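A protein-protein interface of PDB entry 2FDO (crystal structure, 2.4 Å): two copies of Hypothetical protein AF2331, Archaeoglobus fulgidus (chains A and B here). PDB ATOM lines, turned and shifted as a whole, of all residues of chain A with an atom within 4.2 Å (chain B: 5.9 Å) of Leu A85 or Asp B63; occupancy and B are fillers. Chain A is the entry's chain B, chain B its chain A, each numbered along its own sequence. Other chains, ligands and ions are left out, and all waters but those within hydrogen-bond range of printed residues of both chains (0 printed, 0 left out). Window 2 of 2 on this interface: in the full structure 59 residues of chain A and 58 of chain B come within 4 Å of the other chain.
The backbone NH (N) of Gly A89 lies within hydrogen-bond range of the side-chain hydroxyl (OG) of Ser A86.
Hydrophobic or aromatic side chains of chain B that line the printed part of chain A: Val B26, Val B28, Ile B61 and Phe B62. Of the 10 printed residues of chain A, 6 touch a printed residue of chain B. Hydrophobic or aromatic side chains of chain A within 4 Å of the printed part of chain B: Val A80 and Leu A85.
No position is printed for both chains. Of the 13 pairs that touch across the chains among the printed residues, none has its exchanged pair printed and touching as well.
Of chain B, only Val B26 (3.8 Å), Ile B61 (3.2 Å) and Asp B63 (3.3 Å) come within 4 Å of Leu A85. Of the printed residues of chain A, Ile B61 touches Leu A85, Ser A86 and Gly A89. Of the printed residues of chain B, Lys A82 touches Val B26. Printed residues of chain A within 4 Å of Val B28: Val A80. Of the printed residues of chain B, Gly A89 touches Ile B61. Arg A90 touches none of the printed residues of chain B. The nearest residue of chain B that does not touch Leu A85 is Phe B62 (4.2 Å). The nearest printed residue of chain A that does not touch Asp B63 is Glu A83 (4.5 Å). The nearest printed residue of chain A that does not touch Val B26 is Ile A93 (4.2 Å).
Val A80 touches Val B28 (CG2 to CG2, 3.5 Å). CE2 of Phe B62 touches CG2 of Val A80 (3.7 Å). Lys A82 touches Val B26. Phe B62 touches Lys A84 (CA to O, 3.4 Å). CG2 of Val B26 touches CD1 of Leu A85, at 3.8 Å. Leu A85 touches Ile B61. O of Leu A85 touches CB of Asp B63 (3.3 Å). Phe B62 touches Ser A86 (C to N, 3.7 Å). Asp B63 touches Ser A86. Gly A89 touches Ile B61 (CA to O, 3.5 Å).
The backbone NH (N) of Val B26 lies within hydrogen-bond range of the backbone carbonyl oxygen (O) of Val A80 (2.7 Å). The backbone carbonyl oxygen (O) of Lys A84 is in hydrogen-bond range of the backbone NH (N) of Asp B63. The backbone carbonyl oxygen of Ile B61 lies within hydrogen-bond range of the backbone NH of Ser A86 (2.7 Å).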
ATOM      1  N   VAL A  80     -13.118  -0.413 -23.280  1.00  0.00           N
ATOM      2  CA  VAL A  80     -13.283  -0.635 -24.704  1.00  0.00           C
ATOM      3  C   VAL A  80     -11.899  -0.615 -25.324  1.00  0.00           C
ATOM      4  O   VAL A  80     -11.215   0.424 -25.287  1.00  0.00           O
ATOM      5  CB  VAL A  80     -14.082   0.534 -25.340  1.00  0.00           C
ATOM      6  CG1 VAL A  80     -14.369   0.250 -26.803  1.00  0.00           C
ATOM      7  CG2 VAL A  80     -15.396   0.775 -24.572  1.00  0.00           C
ATOM      8  N   GLU A  81     -11.467  -1.751 -25.863  1.00  0.00           N
ATOM      9  CA  GLU A  81     -10.283  -1.788 -26.706  1.00  0.00           C
ATOM     10  C   GLU A  81     -10.404  -0.786 -27.854  1.00  0.00           C
ATOM     11  O   GLU A  81     -11.497  -0.598 -28.402  1.00  0.00           O
ATOM     12  CB  GLU A  81     -10.115  -3.179 -27.297  1.00  0.00           C
ATOM     13  CG  GLU A  81      -9.506  -4.179 -26.369  1.00  0.00           C
ATOM     14  CD  GLU A  81     -10.524  -5.185 -25.898  1.00  0.00           C
ATOM     15  OE1 GLU A  81     -11.693  -4.784 -25.594  1.00  0.00           O
ATOM     16  OE2 GLU A  81     -10.150  -6.396 -25.852  1.00  0.00           O
ATOM     17  N   LYS A  82      -9.289  -0.168 -28.230  1.00  0.00           N
ATOM     18  CA  LYS A  82      -9.285   0.846 -29.305  1.00  0.00           C
ATOM     19  C   LYS A  82      -9.729   0.393 -30.719  1.00  0.00           C
ATOM     20  O   LYS A  82     -10.365   1.171 -31.435  1.00  0.00           O
ATOM     21  CB  LYS A  82      -7.935   1.593 -29.380  1.00  0.00           C
ATOM     22  CG  LYS A  82      -7.574   2.437 -28.133  1.00  0.00           C
ATOM     23  CD  LYS A  82      -6.518   3.461 -28.512  1.00  0.00           C
ATOM     24  CE  LYS A  82      -5.835   4.074 -27.295  1.00  0.00           C
ATOM     25  NZ  LYS A  82      -4.393   3.678 -27.252  1.00  0.00           N
ATOM     26  N   GLU A  83      -9.371  -0.826 -31.121  1.00  0.00           N
ATOM     27  CA  GLU A  83      -9.955  -1.497 -32.311  1.00  0.00           C
ATOM     28  C   GLU A  83     -11.510  -1.507 -32.383  1.00  0.00           C
ATOM     29  O   GLU A  83     -12.083  -1.685 -33.451  1.00  0.00           O
ATOM     30  CB  GLU A  83      -9.463  -2.941 -32.366  1.00  0.00           C
ATOM     31  CG  GLU A  83      -8.064  -3.092 -32.951  1.00  0.00           C
ATOM     32  N   LYS A  84     -12.190  -1.329 -31.256  1.00  0.00           N
ATOM     33  CA  LYS A  84     -13.645  -1.407 -31.243  1.00  0.00           C
ATOM     34  C   LYS A  84     -14.361  -0.041 -31.285  1.00  0.00           C
ATOM     35  O   LYS A  84     -15.573   0.034 -31.105  1.00  0.00           O
ATOM     36  CB  LYS A  84     -14.124  -2.300 -30.074  1.00  0.00           C
ATOM     37  CG  LYS A  84     -13.794  -3.828 -30.296  1.00  0.00           C
ATOM     38  N   LEU A  85     -13.620   1.029 -31.553  1.00  0.00           N
ATOM     39  CA  LEU A  85     -14.214   2.361 -31.722  1.00  0.00           C
ATOM     40  C   LEU A  85     -14.508   2.639 -33.206  1.00  0.00           C
ATOM     41  O   LEU A  85     -13.802   2.155 -34.087  1.00  0.00           O
ATOM     42  CB  LEU A  85     -13.252   3.460 -31.197  1.00  0.00           C
ATOM     43  CG  LEU A  85     -12.837   3.404 -29.713  1.00  0.00           C
ATOM     44  CD1 LEU A  85     -11.743   4.384 -29.352  1.00  0.00           C
ATOM     45  CD2 LEU A  85     -14.042   3.586 -28.798  1.00  0.00           C
ATOM     46  N   SER A  86     -15.528   3.442 -33.473  1.00  0.00           N
ATOM     47  CA  SER A  86     -15.661   4.097 -34.766  1.00  0.00           C
ATOM     48  C   SER A  86     -14.648   5.259 -34.893  1.00  0.00           C
ATOM     49  O   SER A  86     -13.920   5.603 -33.932  1.00  0.00           O
ATOM     50  CB  SER A  86     -17.060   4.695 -34.857  1.00  0.00           C
ATOM     51  OG  SER A  86     -17.184   5.701 -33.845  1.00  0.00           O
ATOM     52  N   GLY A  89     -15.789   7.588 -32.313  1.00  0.00           N
ATOM     53  CA  GLY A  89     -15.310   7.192 -30.994  1.00  0.00           C
ATOM     54  C   GLY A  89     -13.849   7.550 -30.784  1.00  0.00           C
ATOM     55  O   GLY A  89     -13.443   7.852 -29.672  1.00  0.00           O
ATOM     56  N   ARG A  90     -13.074   7.507 -31.869  1.00  0.00           N
ATOM     57  CA  ARG A  90     -11.680   7.955 -31.866  1.00  0.00           C
ATOM     58  C   ARG A  90     -11.574   9.477 -31.734  1.00  0.00           C
ATOM     59  O   ARG A  90     -10.750   9.971 -30.962  1.00  0.00           O
ATOM     60  CB  ARG A  90     -10.956   7.480 -33.117  1.00  0.00           C
ATOM     61  CG  ARG A  90     -10.366   6.077 -33.033  1.00  0.00           C
ATOM     62  N   ILE A  93     -11.908  10.834 -27.931  1.00  0.00           N
ATOM     63  CA  ILE A  93     -11.053  10.390 -26.842  1.00  0.00           C
ATOM     64  C   ILE A  93     -10.402  11.599 -26.194  1.00  0.00           C
ATOM     65  O   ILE A  93      -9.769  12.375 -26.873  1.00  0.00           O
ATOM     66  CB  ILE A  93      -9.926   9.445 -27.313  1.00  0.00           C
ATOM     67  CG1 ILE A  93     -10.517   8.127 -27.821  1.00  0.00           C
ATOM     68  CG2 ILE A  93      -8.884   9.203 -26.179  1.00  0.00           C
ATOM     69  CD1 ILE A  93      -9.529   7.352 -28.688  1.00  0.00           C
ATOM     70  N   VAL B  26      -9.551   2.146 -24.026  1.00  0.00           N
ATOM     71  CA  VAL B  26     -10.138   3.392 -23.511  1.00  0.00           C
ATOM     72  C   VAL B  26     -11.313   3.110 -22.521  1.00  0.00           C
ATOM     73  O   VAL B  26     -11.697   1.973 -22.329  1.00  0.00           O
ATOM     74  CB  VAL B  26     -10.514   4.381 -24.666  1.00  0.00           C
ATOM     75  CG1 VAL B  26      -9.287   4.710 -25.454  1.00  0.00           C
ATOM     76  CG2 VAL B  26     -11.615   3.799 -25.571  1.00  0.00           C
ATOM     77  N   VAL B  28     -15.162   4.214 -21.707  1.00  0.00           N
ATOM     78  CA  VAL B  28     -16.390   4.941 -21.926  1.00  0.00           C
ATOM     79  C   VAL B  28     -17.109   5.213 -20.586  1.00  0.00           C
ATOM     80  O   VAL B  28     -17.376   4.304 -19.793  1.00  0.00           O
ATOM     81  CB  VAL B  28     -17.259   4.198 -22.959  1.00  0.00           C
ATOM     82  CG1 VAL B  28     -18.637   4.865 -23.136  1.00  0.00           C
ATOM     83  CG2 VAL B  28     -16.481   4.101 -24.290  1.00  0.00           C
ATOM     84  N   ALA B  59     -24.237   4.716 -29.049  1.00  0.00           N
ATOM     85  CA  ALA B  59     -23.729   3.579 -29.815  1.00  0.00           C
ATOM     86  C   ALA B  59     -22.776   3.983 -30.948  1.00  0.00           C
ATOM     87  O   ALA B  59     -21.899   3.199 -31.314  1.00  0.00           O
ATOM     88  CB  ALA B  59     -24.876   2.774 -30.379  1.00  0.00           C
ATOM     89  N   ILE B  61     -20.173   5.537 -31.237  1.00  0.00           N
ATOM     90  CA  ILE B  61     -18.737   5.588 -30.947  1.00  0.00           C
ATOM     91  C   ILE B  61     -18.094   4.195 -31.132  1.00  0.00           C
ATOM     92  O   ILE B  61     -16.860   4.047 -31.204  1.00  0.00           O
ATOM     93  CB  ILE B  61     -18.428   6.172 -29.540  1.00  0.00           C
ATOM     94  CG1 ILE B  61     -19.054   5.302 -28.449  1.00  0.00           C
ATOM     95  CG2 ILE B  61     -18.820   7.664 -29.494  1.00  0.00           C
ATOM     96  CD1 ILE B  61     -18.856   5.757 -27.041  1.00  0.00           C
ATOM     97  N   PHE B  62     -18.950   3.187 -31.240  1.00  0.00           N
ATOM     98  CA  PHE B  62     -18.485   1.818 -31.346  1.00  0.00           C
ATOM     99  C   PHE B  62     -18.456   1.324 -32.774  1.00  0.00           C
ATOM    100  O   PHE B  62     -19.280   1.713 -33.603  1.00  0.00           O
ATOM    101  CB  PHE B  62     -19.397   0.908 -30.540  1.00  0.00           C
ATOM    102  CG  PHE B  62     -19.304   1.107 -29.052  1.00  0.00           C
ATOM    103  CD1 PHE B  62     -20.304   1.779 -28.376  1.00  0.00           C
ATOM    104  CD2 PHE B  62     -18.238   0.591 -28.338  1.00  0.00           C
ATOM    105  CE1 PHE B  62     -20.261   1.923 -27.028  1.00  0.00           C
ATOM    106  CE2 PHE B  62     -18.164   0.759 -26.985  1.00  0.00           C
ATOM    107  CZ  PHE B  62     -19.193   1.417 -26.315  1.00  0.00           C
ATOM    108  N   ASP B  63     -17.498   0.451 -33.046  1.00  0.00           N
ATOM    109  CA  ASP B  63     -17.442  -0.288 -34.293  1.00  0.00           C
ATOM    110  C   ASP B  63     -17.664  -1.714 -33.835  1.00  0.00           C
ATOM    111  O   ASP B  63     -16.740  -2.527 -33.814  1.00  0.00           O
ATOM    112  CB  ASP B  63     -16.058  -0.121 -34.931  1.00  0.00           C
ATOM    113  CG  ASP B  63     -16.041  -0.416 -36.423  1.00  0.00           C
ATOM    114  OD1 ASP B  63     -16.823  -1.284 -36.890  1.00  0.00           O
ATOM    115  OD2 ASP B  63     -15.220   0.232 -37.132  1.00  0.00           O
ATOM    116  N   ALA B  64     -18.902  -2.007 -33.456  1.00  0.00           N
ATOM    117  CA  ALA B  64     -19.217  -3.245 -32.761  1.00  0.00           C
ATOM    118  C   ALA B  64     -20.728  -3.452 -32.730  1.00  0.00           C
ATOM    119  O   ALA B  64     -21.464  -2.485 -32.550  1.00  0.00           O
ATOM    120  CB  ALA B  64     -18.657  -3.183 -31.327  1.00  0.00           C
ATOM    121  N   ASP B  65     -21.201  -4.692 -32.866  1.00  0.00           N
ATOM    122  CA  ASP B  65     -22.630  -4.927 -32.708  1.00  0.00           C
ATOM    123  C   ASP B  65     -23.066  -4.961 -31.234  1.00  0.00           C
ATOM    124  O   ASP B  65     -22.255  -4.749 -30.331  1.00  0.00           O
ATOM    125  CB  ASP B  65     -23.150  -6.117 -33.550  1.00  0.00           C
ATOM    126  CG  ASP B  65     -22.551  -7.478 -33.147  1.00  0.00           C
ATOM    127  OD1 ASP B  65     -22.390  -7.776 -31.925  1.00  0.00           O
ATOM    128  OD2 ASP B  65     -22.288  -8.280 -34.092  1.00  0.00           O
ATOM    129  N   GLU B  68     -21.383  -7.659 -28.927  1.00  0.00           N
ATOM    130  CA  GLU B  68     -20.019  -7.244 -28.591  1.00  0.00           C
ATOM    131  C   GLU B  68     -19.939  -6.159 -27.501  1.00  0.00           C
ATOM    132  O   GLU B  68     -19.128  -6.263 -26.596  1.00  0.00           O
ATOM    133  CB  GLU B  68     -19.242  -6.843 -29.848  1.00  0.00           C
ATOM    134  CG  GLU B  68     -19.059  -8.030 -30.763  1.00  0.00           C
ATOM    135  CD  GLU B  68     -18.928  -7.650 -32.232  1.00  0.00           C
ATOM    136  OE1 GLU B  68     -18.217  -6.668 -32.557  1.00  0.00           O
ATOM    137  OE2 GLU B  68     -19.533  -8.370 -33.072  1.00  0.00           O
